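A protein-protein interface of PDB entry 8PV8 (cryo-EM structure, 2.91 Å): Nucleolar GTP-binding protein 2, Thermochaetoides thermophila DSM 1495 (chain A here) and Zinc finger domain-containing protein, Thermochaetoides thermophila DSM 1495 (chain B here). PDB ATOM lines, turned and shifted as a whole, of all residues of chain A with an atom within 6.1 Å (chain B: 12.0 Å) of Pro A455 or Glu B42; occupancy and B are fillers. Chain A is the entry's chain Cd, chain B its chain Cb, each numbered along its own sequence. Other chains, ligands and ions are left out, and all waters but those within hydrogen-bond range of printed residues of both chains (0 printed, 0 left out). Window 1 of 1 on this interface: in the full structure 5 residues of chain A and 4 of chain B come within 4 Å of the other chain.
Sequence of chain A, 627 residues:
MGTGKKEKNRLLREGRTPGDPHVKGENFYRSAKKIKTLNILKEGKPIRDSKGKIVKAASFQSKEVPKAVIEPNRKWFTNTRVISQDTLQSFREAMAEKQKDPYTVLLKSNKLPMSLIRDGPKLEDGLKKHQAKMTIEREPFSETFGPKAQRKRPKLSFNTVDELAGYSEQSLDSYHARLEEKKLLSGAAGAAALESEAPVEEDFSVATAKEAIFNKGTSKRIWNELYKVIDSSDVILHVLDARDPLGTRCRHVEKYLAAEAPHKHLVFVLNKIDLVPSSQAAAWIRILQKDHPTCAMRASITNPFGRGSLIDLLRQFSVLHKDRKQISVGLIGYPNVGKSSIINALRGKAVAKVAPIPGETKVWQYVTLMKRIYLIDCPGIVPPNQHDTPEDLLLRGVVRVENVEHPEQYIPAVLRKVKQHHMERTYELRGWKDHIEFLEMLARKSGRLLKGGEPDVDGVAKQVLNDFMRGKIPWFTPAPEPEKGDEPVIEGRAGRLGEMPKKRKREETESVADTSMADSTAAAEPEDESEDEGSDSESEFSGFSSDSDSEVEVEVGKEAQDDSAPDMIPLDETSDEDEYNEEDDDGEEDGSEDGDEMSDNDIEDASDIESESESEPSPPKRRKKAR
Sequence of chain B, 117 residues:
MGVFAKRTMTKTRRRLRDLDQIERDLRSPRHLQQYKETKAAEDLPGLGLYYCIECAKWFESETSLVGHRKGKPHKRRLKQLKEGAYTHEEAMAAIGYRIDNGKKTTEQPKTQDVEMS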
ATOM      1  N   LEU A 439       0.473  31.890  17.514  1.00  0.00           N
ATOM      2  CA  LEU A 439       1.789  32.491  17.700  1.00  0.00           C
ATOM      3  C   LEU A 439       2.834  31.445  18.071  1.00  0.00           C
ATOM      4  O   LEU A 439       3.981  31.528  17.623  1.00  0.00           O
ATOM      5  CB  LEU A 439       1.730  33.588  18.763  1.00  0.00           C
ATOM      6  CG  LEU A 439       0.863  34.814  18.469  1.00  0.00           C
ATOM      7  CD1 LEU A 439       0.831  35.744  19.668  1.00  0.00           C
ATOM      8  CD2 LEU A 439       1.335  35.549  17.228  1.00  0.00           C
ATOM      9  N   GLU A 440       2.453  30.447  18.876  1.00  0.00           N
ATOM     10  CA  GLU A 440       3.400  29.398  19.249  1.00  0.00           C
ATOM     11  C   GLU A 440       3.801  28.547  18.047  1.00  0.00           C
ATOM     12  O   GLU A 440       4.986  28.235  17.871  1.00  0.00           O
ATOM     13  CB  GLU A 440       2.809  28.524  20.354  1.00  0.00           C
ATOM     14  CG  GLU A 440       2.803  29.184  21.721  1.00  0.00           C
ATOM     15  CD  GLU A 440       1.902  28.471  22.707  1.00  0.00           C
ATOM     16  OE1 GLU A 440       1.034  27.691  22.266  1.00  0.00           O
ATOM     17  OE2 GLU A 440       2.060  28.693  23.927  1.00  0.00           O
ATOM     18  N   ALA A 443       6.086  30.613  15.873  1.00  0.00           N
ATOM     19  CA  ALA A 443       7.412  30.719  16.472  1.00  0.00           C
ATOM     20  C   ALA A 443       8.215  29.440  16.278  1.00  0.00           C
ATOM     21  O   ALA A 443       9.400  29.487  15.927  1.00  0.00           O
ATOM     22  CB  ALA A 443       7.288  31.051  17.958  1.00  0.00           C
ATOM     23  N   ARG A 444       7.585  28.282  16.497  1.00  0.00           N
ATOM     24  CA  ARG A 444       8.301  27.021  16.330  1.00  0.00           C
ATOM     25  C   ARG A 444       8.630  26.756  14.867  1.00  0.00           C
ATOM     26  O   ARG A 444       9.647  26.123  14.562  1.00  0.00           O
ATOM     27  CB  ARG A 444       7.492  25.864  16.918  1.00  0.00           C
ATOM     28  CG  ARG A 444       7.223  25.993  18.404  1.00  0.00           C
ATOM     29  CD  ARG A 444       6.591  24.736  18.969  1.00  0.00           C
ATOM     30  NE  ARG A 444       5.844  25.020  20.188  1.00  0.00           N
ATOM     31  CZ  ARG A 444       4.531  25.201  20.232  1.00  0.00           C
ATOM     32  NH1 ARG A 444       3.784  25.105  19.145  1.00  0.00           N
ATOM     33  NH2 ARG A 444       3.954  25.487  21.395  1.00  0.00           N
ATOM     34  N   ARG A 448      11.769  31.219  15.990  1.00  0.00           N
ATOM     35  CA  ARG A 448      11.792  32.264  17.012  1.00  0.00           C
ATOM     36  C   ARG A 448      11.719  31.611  18.392  1.00  0.00           C
ATOM     37  O   ARG A 448      10.679  31.562  19.051  1.00  0.00           O
ATOM     38  CB  ARG A 448      10.655  33.252  16.793  1.00  0.00           C
ATOM     39  CG  ARG A 448      10.712  33.998  15.468  1.00  0.00           C
ATOM     40  CD  ARG A 448      11.584  35.249  15.542  1.00  0.00           C
ATOM     41  NE  ARG A 448      13.012  34.954  15.492  1.00  0.00           N
ATOM     42  CZ  ARG A 448      13.683  34.658  14.388  1.00  0.00           C
ATOM     43  NH1 ARG A 448      13.090  34.616  13.207  1.00  0.00           N
ATOM     44  NH2 ARG A 448      14.984  34.394  14.472  1.00  0.00           N
ATOM     45  N   LEU A 449      12.865  31.097  18.823  1.00  0.00           N
ATOM     46  CA  LEU A 449      12.988  30.384  20.083  1.00  0.00           C
ATOM     47  C   LEU A 449      13.973  31.100  20.994  1.00  0.00           C
ATOM     48  O   LEU A 449      15.033  31.556  20.557  1.00  0.00           O
ATOM     49  CB  LEU A 449      13.447  28.942  19.855  1.00  0.00           C
ATOM     50  CG  LEU A 449      12.644  28.140  18.831  1.00  0.00           C
ATOM     51  CD1 LEU A 449      13.265  26.772  18.617  1.00  0.00           C
ATOM     52  CD2 LEU A 449      11.197  28.012  19.273  1.00  0.00           C
ATOM     53  N   LEU A 450      13.610  31.196  22.267  1.00  0.00           N
ATOM     54  CA  LEU A 450      14.464  31.793  23.279  1.00  0.00           C
ATOM     55  C   LEU A 450      15.397  30.737  23.859  1.00  0.00           C
ATOM     56  O   LEU A 450      15.431  29.587  23.414  1.00  0.00           O
ATOM     57  CB  LEU A 450      13.621  32.434  24.384  1.00  0.00           C
ATOM     58  CG  LEU A 450      12.590  33.468  23.927  1.00  0.00           C
ATOM     59  CD1 LEU A 450      11.714  33.902  25.087  1.00  0.00           C
ATOM     60  CD2 LEU A 450      13.276  34.666  23.296  1.00  0.00           C
ATOM     61  N   GLY A 453      14.554  26.677  24.582  1.00  0.00           N
ATOM     62  CA  GLY A 453      13.538  26.159  23.679  1.00  0.00           C
ATOM     63  C   GLY A 453      12.175  26.793  23.834  1.00  0.00           C
ATOM     64  O   GLY A 453      11.179  26.222  23.379  1.00  0.00           O
ATOM     65  N   GLU A 454      12.101  27.959  24.462  1.00  0.00           N
ATOM     66  CA  GLU A 454      10.825  28.636  24.662  1.00  0.00           C
ATOM     67  C   GLU A 454      10.488  29.486  23.443  1.00  0.00           C
ATOM     68  O   GLU A 454      11.338  30.262  22.987  1.00  0.00           O
ATOM     69  CB  GLU A 454      10.867  29.511  25.906  1.00  0.00           C
ATOM     70  CG  GLU A 454       9.617  30.344  26.125  1.00  0.00           C
ATOM     71  CD  GLU A 454       9.702  31.204  27.367  1.00  0.00           C
ATOM     72  OE1 GLU A 454      10.661  31.029  28.148  1.00  0.00           O
ATOM     73  OE2 GLU A 454       8.811  32.056  27.565  1.00  0.00           O
ATOM     74  N   PRO A 455       9.287  29.348  22.880  1.00  0.00           N
ATOM     75  CA  PRO A 455       8.912  30.156  21.711  1.00  0.00           C
ATOM     76  C   PRO A 455       8.820  31.639  22.047  1.00  0.00           C
ATOM     77  O   PRO A 455       8.451  32.021  23.160  1.00  0.00           O
ATOM     78  CB  PRO A 455       7.548  29.581  21.309  1.00  0.00           C
ATOM     79  CG  PRO A 455       7.041  28.896  22.530  1.00  0.00           C
ATOM     80  CD  PRO A 455       8.250  28.361  23.224  1.00  0.00           C
ATOM     81  N   ASP A 456       9.158  32.477  21.064  1.00  0.00           N
ATOM     82  CA  ASP A 456       9.151  33.932  21.233  1.00  0.00           C
ATOM     83  C   ASP A 456       7.822  34.479  20.722  1.00  0.00           C
ATOM     84  O   ASP A 456       7.710  35.025  19.619  1.00  0.00           O
ATOM     85  CB  ASP A 456      10.336  34.562  20.511  1.00  0.00           C
ATOM     86  CG  ASP A 456      10.478  36.041  20.806  1.00  0.00           C
ATOM     87  OD1 ASP A 456       9.932  36.502  21.831  1.00  0.00           O
ATOM     88  OD2 ASP A 456      11.135  36.746  20.012  1.00  0.00           O
ATOM     89  N   VAL A 457       6.795  34.336  21.567  1.00  0.00           N
ATOM     90  CA  VAL A 457       5.450  34.770  21.201  1.00  0.00           C
ATOM     91  C   VAL A 457       5.388  36.285  21.059  1.00  0.00           C
ATOM     92  O   VAL A 457       4.671  36.807  20.201  1.00  0.00           O
ATOM     93  CB  VAL A 457       4.419  34.246  22.220  1.00  0.00           C
ATOM     94  CG1 VAL A 457       4.183  32.762  22.010  1.00  0.00           C
ATOM     95  CG2 VAL A 457       4.889  34.498  23.644  1.00  0.00           C
ATOM     96  N   ASP A 458       6.152  37.014  21.882  1.00  0.00           N
ATOM     97  CA  ASP A 458       6.172  38.473  21.789  1.00  0.00           C
ATOM     98  C   ASP A 458       6.764  38.938  20.463  1.00  0.00           C
ATOM     99  O   ASP A 458       6.189  39.801  19.785  1.00  0.00           O
ATOM    100  CB  ASP A 458       6.964  39.059  22.956  1.00  0.00           C
ATOM    101  CG  ASP A 458       6.264  38.877  24.286  1.00  0.00           C
ATOM    102  OD1 ASP A 458       5.018  38.828  24.302  1.00  0.00           O
ATOM    103  OD2 ASP A 458       6.963  38.783  25.317  1.00  0.00           O
ATOM    104  N   TYR B  35       6.432  18.315  40.478  1.00  0.00           N
ATOM    105  CA  TYR B  35       7.519  19.056  39.841  1.00  0.00           C
ATOM    106  C   TYR B  35       7.150  19.475  38.420  1.00  0.00           C
ATOM    107  O   TYR B  35       7.542  20.551  37.956  1.00  0.00           O
ATOM    108  CB  TYR B  35       8.805  18.233  39.837  1.00  0.00           C
ATOM    109  CG  TYR B  35       9.943  18.921  39.109  1.00  0.00           C
ATOM    110  CD1 TYR B  35      10.348  20.200  39.470  1.00  0.00           C
ATOM    111  CD2 TYR B  35      10.607  18.295  38.063  1.00  0.00           C
ATOM    112  CE1 TYR B  35      11.384  20.838  38.811  1.00  0.00           C
ATOM    113  CE2 TYR B  35      11.647  18.925  37.397  1.00  0.00           C
ATOM    114  CZ  TYR B  35      12.029  20.196  37.777  1.00  0.00           C
ATOM    115  OH  TYR B  35      13.061  20.827  37.118  1.00  0.00           O
ATOM    116  N   LYS B  36       6.388  18.640  37.714  1.00  0.00           N
ATOM    117  CA  LYS B  36       5.967  18.999  36.365  1.00  0.00           C
ATOM    118  C   LYS B  36       4.826  20.011  36.350  1.00  0.00           C
ATOM    119  O   LYS B  36       4.774  20.846  35.442  1.00  0.00           O
ATOM    120  CB  LYS B  36       5.575  17.747  35.582  1.00  0.00           C
ATOM    121  CG  LYS B  36       6.761  16.875  35.210  1.00  0.00           C
ATOM    122  CD  LYS B  36       6.356  15.783  34.240  1.00  0.00           C
ATOM    123  CE  LYS B  36       7.567  15.023  33.733  1.00  0.00           C
ATOM    124  NZ  LYS B  36       7.189  13.956  32.767  1.00  0.00           N
ATOM    125  N   GLU B  37       3.913  19.961  37.325  1.00  0.00           N
ATOM    126  CA  GLU B  37       2.882  20.988  37.430  1.00  0.00           C
ATOM    127  C   GLU B  37       3.442  22.325  37.888  1.00  0.00           C
ATOM    128  O   GLU B  37       2.775  23.352  37.715  1.00  0.00           O
ATOM    129  CB  GLU B  37       1.766  20.547  38.380  1.00  0.00           C
ATOM    130  CG  GLU B  37       0.949  19.362  37.891  1.00  0.00           C
ATOM    131  CD  GLU B  37       0.128  19.685  36.658  1.00  0.00           C
ATOM    132  OE1 GLU B  37      -0.304  20.849  36.513  1.00  0.00           O
ATOM    133  OE2 GLU B  37      -0.086  18.775  35.830  1.00  0.00           O
ATOM    134  N   THR B  38       4.632  22.334  38.485  1.00  0.00           N
ATOM    135  CA  THR B  38       5.330  23.580  38.780  1.00  0.00           C
ATOM    136  C   THR B  38       5.638  24.394  37.521  1.00  0.00           C
ATOM    137  O   THR B  38       5.504  25.622  37.545  1.00  0.00           O
ATOM    138  CB  THR B  38       6.626  23.277  39.550  1.00  0.00           C
ATOM    139  OG1 THR B  38       6.303  22.609  40.777  1.00  0.00           O
ATOM    140  CG2 THR B  38       7.394  24.550  39.879  1.00  0.00           C
ATOM    141  N   LYS B  39       5.988  23.743  36.412  1.00  0.00           N
ATOM    142  CA  LYS B  39       6.388  24.420  35.184  1.00  0.00           C
ATOM    143  C   LYS B  39       5.211  24.509  34.221  1.00  0.00           C
ATOM    144  O   LYS B  39       4.331  23.644  34.220  1.00  0.00           O
ATOM    145  CB  LYS B  39       7.553  23.684  34.505  1.00  0.00           C
ATOM    146  CG  LYS B  39       8.738  23.369  35.413  1.00  0.00           C
ATOM    147  CD  LYS B  39       9.215  24.580  36.204  1.00  0.00           C
ATOM    148  CE  LYS B  39       9.905  25.596  35.307  1.00  0.00           C
ATOM    149  NZ  LYS B  39      11.289  25.169  34.959  1.00  0.00           N
ATOM    150  N   ALA B  40       5.198  25.560  33.399  1.00  0.00           N
ATOM    151  CA  ALA B  40       4.160  25.744  32.387  1.00  0.00           C
ATOM    152  C   ALA B  40       4.611  25.077  31.095  1.00  0.00           C
ATOM    153  O   ALA B  40       5.554  25.546  30.453  1.00  0.00           O
ATOM    154  CB  ALA B  40       3.881  27.225  32.155  1.00  0.00           C
ATOM    155  N   ALA B  41       3.873  24.041  30.675  1.00  0.00           N
ATOM    156  CA  ALA B  41       4.369  23.075  29.693  1.00  0.00           C
ATOM    157  C   ALA B  41       4.630  23.691  28.322  1.00  0.00           C
ATOM    158  O   ALA B  41       5.363  23.117  27.508  1.00  0.00           O
ATOM    159  CB  ALA B  41       3.379  21.915  29.569  1.00  0.00           C
ATOM    160  N   GLU B  42       4.040  24.854  28.041  1.00  0.00           N
ATOM    161  CA  GLU B  42       4.232  25.481  26.738  1.00  0.00           C
ATOM    162  C   GLU B  42       5.611  26.115  26.584  1.00  0.00           C
ATOM    163  O   GLU B  42       6.012  26.424  25.457  1.00  0.00           O
ATOM    164  CB  GLU B  42       3.146  26.531  26.498  1.00  0.00           C
ATOM    165  CG  GLU B  42       1.744  25.955  26.371  1.00  0.00           C
ATOM    166  CD  GLU B  42       1.572  25.099  25.130  1.00  0.00           C
ATOM    167  OE1 GLU B  42       2.228  25.389  24.107  1.00  0.00           O
ATOM    168  OE2 GLU B  42       0.779  24.136  25.178  1.00  0.00           O
ATOM    169  N   ASP B  43       6.344  26.318  27.678  1.00  0.00           N
ATOM    170  CA  ASP B  43       7.619  27.024  27.645  1.00  0.00           C
ATOM    171  C   ASP B  43       8.830  26.105  27.761  1.00  0.00           C
ATOM    172  O   ASP B  43       9.941  26.594  27.983  1.00  0.00           O
ATOM    173  CB  ASP B  43       7.659  28.078  28.759  1.00  0.00           C
ATOM    174  CG  ASP B  43       6.590  29.147  28.593  1.00  0.00           C
ATOM    175  OD1 ASP B  43       5.923  29.166  27.537  1.00  0.00           O
ATOM    176  OD2 ASP B  43       6.414  29.965  29.521  1.00  0.00           O
ATOM    177  N   LEU B  44       8.644  24.797  27.623  1.00  0.00           N
ATOM    178  CA  LEU B  44       9.519  23.631  27.656  1.00  0.00           C
ATOM    179  C   LEU B  44       9.879  23.165  26.251  1.00  0.00           C
ATOM    180  O   LEU B  44       9.073  23.308  25.325  1.00  0.00           O
ATOM    181  CB  LEU B  44       8.854  22.483  28.419  1.00  0.00           C
ATOM    182  CG  LEU B  44       8.838  22.492  29.950  1.00  0.00           C
ATOM    183  CD1 LEU B  44       7.940  23.511  30.558  1.00  0.00           C
ATOM    184  CD2 LEU B  44       8.329  21.149  30.367  1.00  0.00           C
ATOM    185  N   PRO B  45      11.087  22.626  26.075  1.00  0.00           N
ATOM    186  CA  PRO B  45      11.479  22.103  24.759  1.00  0.00           C
ATOM    187  C   PRO B  45      10.665  20.871  24.393  1.00  0.00           C
ATOM    188  O   PRO B  45      10.538  19.933  25.182  1.00  0.00           O
ATOM    189  CB  PRO B  45      12.962  21.761  24.938  1.00  0.00           C
ATOM    190  CG  PRO B  45      13.404  22.516  26.135  1.00  0.00           C
ATOM    191  CD  PRO B  45      12.213  22.638  27.025  1.00  0.00           C
ATOM    192  N   GLY B  46      10.116  20.880  23.181  1.00  0.00           N
ATOM    193  CA  GLY B  46       9.297  19.772  22.727  1.00  0.00           C
ATOM    194  C   GLY B  46       7.980  19.639  23.456  1.00  0.00           C
ATOM    195  O   GLY B  46       7.417  18.539  23.501  1.00  0.00           O
ATOM    196  N   LEU B  47       7.495  20.735  24.055  1.00  0.00           N
ATOM    197  CA  LEU B  47       6.230  20.790  24.800  1.00  0.00           C
ATOM    198  C   LEU B  47       6.223  19.832  25.992  1.00  0.00           C
ATOM    199  O   LEU B  47       5.171  19.389  26.456  1.00  0.00           O
ATOM    200  CB  LEU B  47       5.031  20.536  23.882  1.00  0.00           C
ATOM    201  CG  LEU B  47       4.795  21.609  22.823  1.00  0.00           C
ATOM    202  CD1 LEU B  47       3.677  21.198  21.881  1.00  0.00           C
ATOM    203  CD2 LEU B  47       4.476  22.927  23.501  1.00  0.00           C
ATOM    204  N   GLY B  48       7.413  19.522  26.504  1.00  0.00           N
ATOM    205  CA  GLY B  48       7.528  18.698  27.694  1.00  0.00           C
ATOM    206  C   GLY B  48       7.200  17.237  27.495  1.00  0.00           C
ATOM    207  O   GLY B  48       6.902  16.539  28.470  1.00  0.00           O
ATOM    208  N   LEU B  49       7.248  16.747  26.257  1.00  0.00           N
ATOM    209  CA  LEU B  49       6.996  15.335  25.996  1.00  0.00           C
ATOM    210  C   LEU B  49       8.245  14.475  26.102  1.00  0.00           C
ATOM    211  O   LEU B  49       8.136  13.245  26.079  1.00  0.00           O
ATOM    212  CB  LEU B  49       6.378  15.133  24.606  1.00  0.00           C
ATOM    213  CG  LEU B  49       4.894  15.420  24.344  1.00  0.00           C
ATOM    214  CD1 LEU B  49       4.558  16.903  24.348  1.00  0.00           C
ATOM    215  CD2 LEU B  49       4.465  14.782  23.029  1.00  0.00           C
ATOM    216  N   TYR B  50       9.421  15.084  26.220  1.00  0.00           N
ATOM    217  CA  TYR B  50      10.686  14.359  26.248  1.00  0.00           C
ATOM    218  C   TYR B  50      11.437  14.789  27.499  1.00  0.00           C
ATOM    219  O   TYR B  50      12.003  15.886  27.541  1.00  0.00           O
ATOM    220  CB  TYR B  50      11.497  14.641  24.985  1.00  0.00           C
ATOM    221  CG  TYR B  50      10.693  14.460  23.719  1.00  0.00           C
ATOM    222  CD1 TYR B  50      10.440  13.196  23.205  1.00  0.00           C
ATOM    223  CD2 TYR B  50      10.178  15.558  23.039  1.00  0.00           C
ATOM    224  CE1 TYR B  50       9.697  13.031  22.052  1.00  0.00           C
ATOM    225  CE2 TYR B  50       9.437  15.402  21.885  1.00  0.00           C
ATOM    226  CZ  TYR B  50       9.201  14.137  21.395  1.00  0.00           C
ATOM    227  OH  TYR B  50       8.465  13.976  20.244  1.00  0.00           O
ATOM    228  N   TRP B  58      14.577  18.527  30.267  1.00  0.00           N
ATOM    229  CA  TRP B  58      13.659  18.416  29.146  1.00  0.00           C
ATOM    230  C   TRP B  58      14.426  18.583  27.840  1.00  0.00           C
ATOM    231  O   TRP B  58      15.350  19.393  27.741  1.00  0.00           O
ATOM    232  CB  TRP B  58      12.545  19.461  29.241  1.00  0.00           C
ATOM    233  CG  TRP B  58      11.507  19.134  30.273  1.00  0.00           C
ATOM    234  CD1 TRP B  58      10.438  18.300  30.127  1.00  0.00           C
ATOM    235  CD2 TRP B  58      11.429  19.656  31.605  1.00  0.00           C
ATOM    236  NE1 TRP B  58       9.708  18.257  31.291  1.00  0.00           N
ATOM    237  CE2 TRP B  58      10.296  19.083  32.214  1.00  0.00           C
ATOM    238  CE3 TRP B  58      12.212  20.548  32.343  1.00  0.00           C
ATOM    239  CZ2 TRP B  58       9.923  19.376  33.523  1.00  0.00           C
ATOM    240  CZ3 TRP B  58      11.841  20.834  33.643  1.00  0.00           C
ATOM    241  CH2 TRP B  58      10.708  20.251  34.220  1.00  0.00           C
ATOM    242  N   PHE B  59      14.035  17.805  26.834  1.00  0.00           N
ATOM    243  CA  PHE B  59      14.738  17.756  25.563  1.00  0.00           C
ATOM    244  C   PHE B  59      13.762  17.996  24.419  1.00  0.00           C
ATOM    245  O   PHE B  59      12.552  17.799  24.553  1.00  0.00           O
ATOM    246  CB  PHE B  59      15.459  16.414  25.377  1.00  0.00           C
ATOM    247  CG  PHE B  59      16.547  16.175  26.380  1.00  0.00           C
ATOM    248  CD1 PHE B  59      16.261  15.602  27.608  1.00  0.00           C
ATOM    249  CD2 PHE B  59      17.851  16.550  26.108  1.00  0.00           C
ATOM    250  CE1 PHE B  59      17.256  15.392  28.537  1.00  0.00           C
ATOM    251  CE2 PHE B  59      18.851  16.344  27.036  1.00  0.00           C
ATOM    252  CZ  PHE B  59      18.551  15.766  28.251  1.00  0.00           C
ATOM    253  N   GLU B  60      14.309  18.438  23.284  1.00  0.00           N
ATOM    254  CA  GLU B  60      13.461  18.872  22.180  1.00  0.00           C
ATOM    255  C   GLU B  60      12.866  17.693  21.417  1.00  0.00           C
ATOM    256  O   GLU B  60      11.789  17.819  20.823  1.00  0.00           O
ATOM    257  CB  GLU B  60      14.247  19.786  21.237  1.00  0.00           C
ATOM    258  CG  GLU B  60      15.397  19.115  20.507  1.00  0.00           C
ATOM    259  CD  GLU B  60      16.180  20.077  19.637  1.00  0.00           C
ATOM    260  OE1 GLU B  60      15.837  21.279  19.621  1.00  0.00           O
ATOM    261  OE2 GLU B  60      17.132  19.632  18.965  1.00  0.00           O
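Of the 19 printed residues of chain B, 3 touch a printed residue of chain A.
Printed residues of chain B that touch a printed residue of chain A: Glu B42, Asp B43 and Leu B47.
Of the 13 printed residues of chain A, 4 touch a printed residue of chain B.
Hydrophobic or aromatic side chains of chain A that line the printed part of chain B: Pro A455.
Among the printed residues, Asp or Glu carboxylates within 4 Å of a Lys or Arg side-chain nitrogen of the other chain: Arg A444 with Glu B42.
OE1 of Glu B42 lies within salt-bridge range of NH2 of Arg A444 (3.2 Å).
The side-chain carboxylate (OE1) of Glu A440 sits close to the side-chain carboxylate (OE1) of Glu B42 (3.2 Å).
Of the printed residues of chain B, Pro A455 touches Glu B42.
Glu B42 touches just these residues of chain A: Glu A440, Arg A444 and Pro A455.
Glu A440 touches one residue of chain B.
No residue of chain B comes within 4 Å of Ala A443.
No residue of chain B comes within 4 Å of Leu A449.
No residue of chain B comes within 4 Å of Leu A450.
No residue of chain B comes within 4 Å of Val A457.
Of the printed residues of chain A, Asp B43 touches Glu A454 (3.7 Å).
Printed residues of chain A within 4 Å of Leu B47: Arg A444 (3.4 Å).
Glu B37 touches none of the printed residues of chain A.
The nearest residue of chain B that does not touch Pro A455 is Asp B43 (4.7 Å).
NH2 of Arg A444 lies within salt-bridge range of OE1 of Glu A440, at 3.8 Å.
Among the printed residues, pairs that only touch across the chains: Arg A444 with Leu B47, Glu A454 with Asp B43 and Pro A455 with Glu B42.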
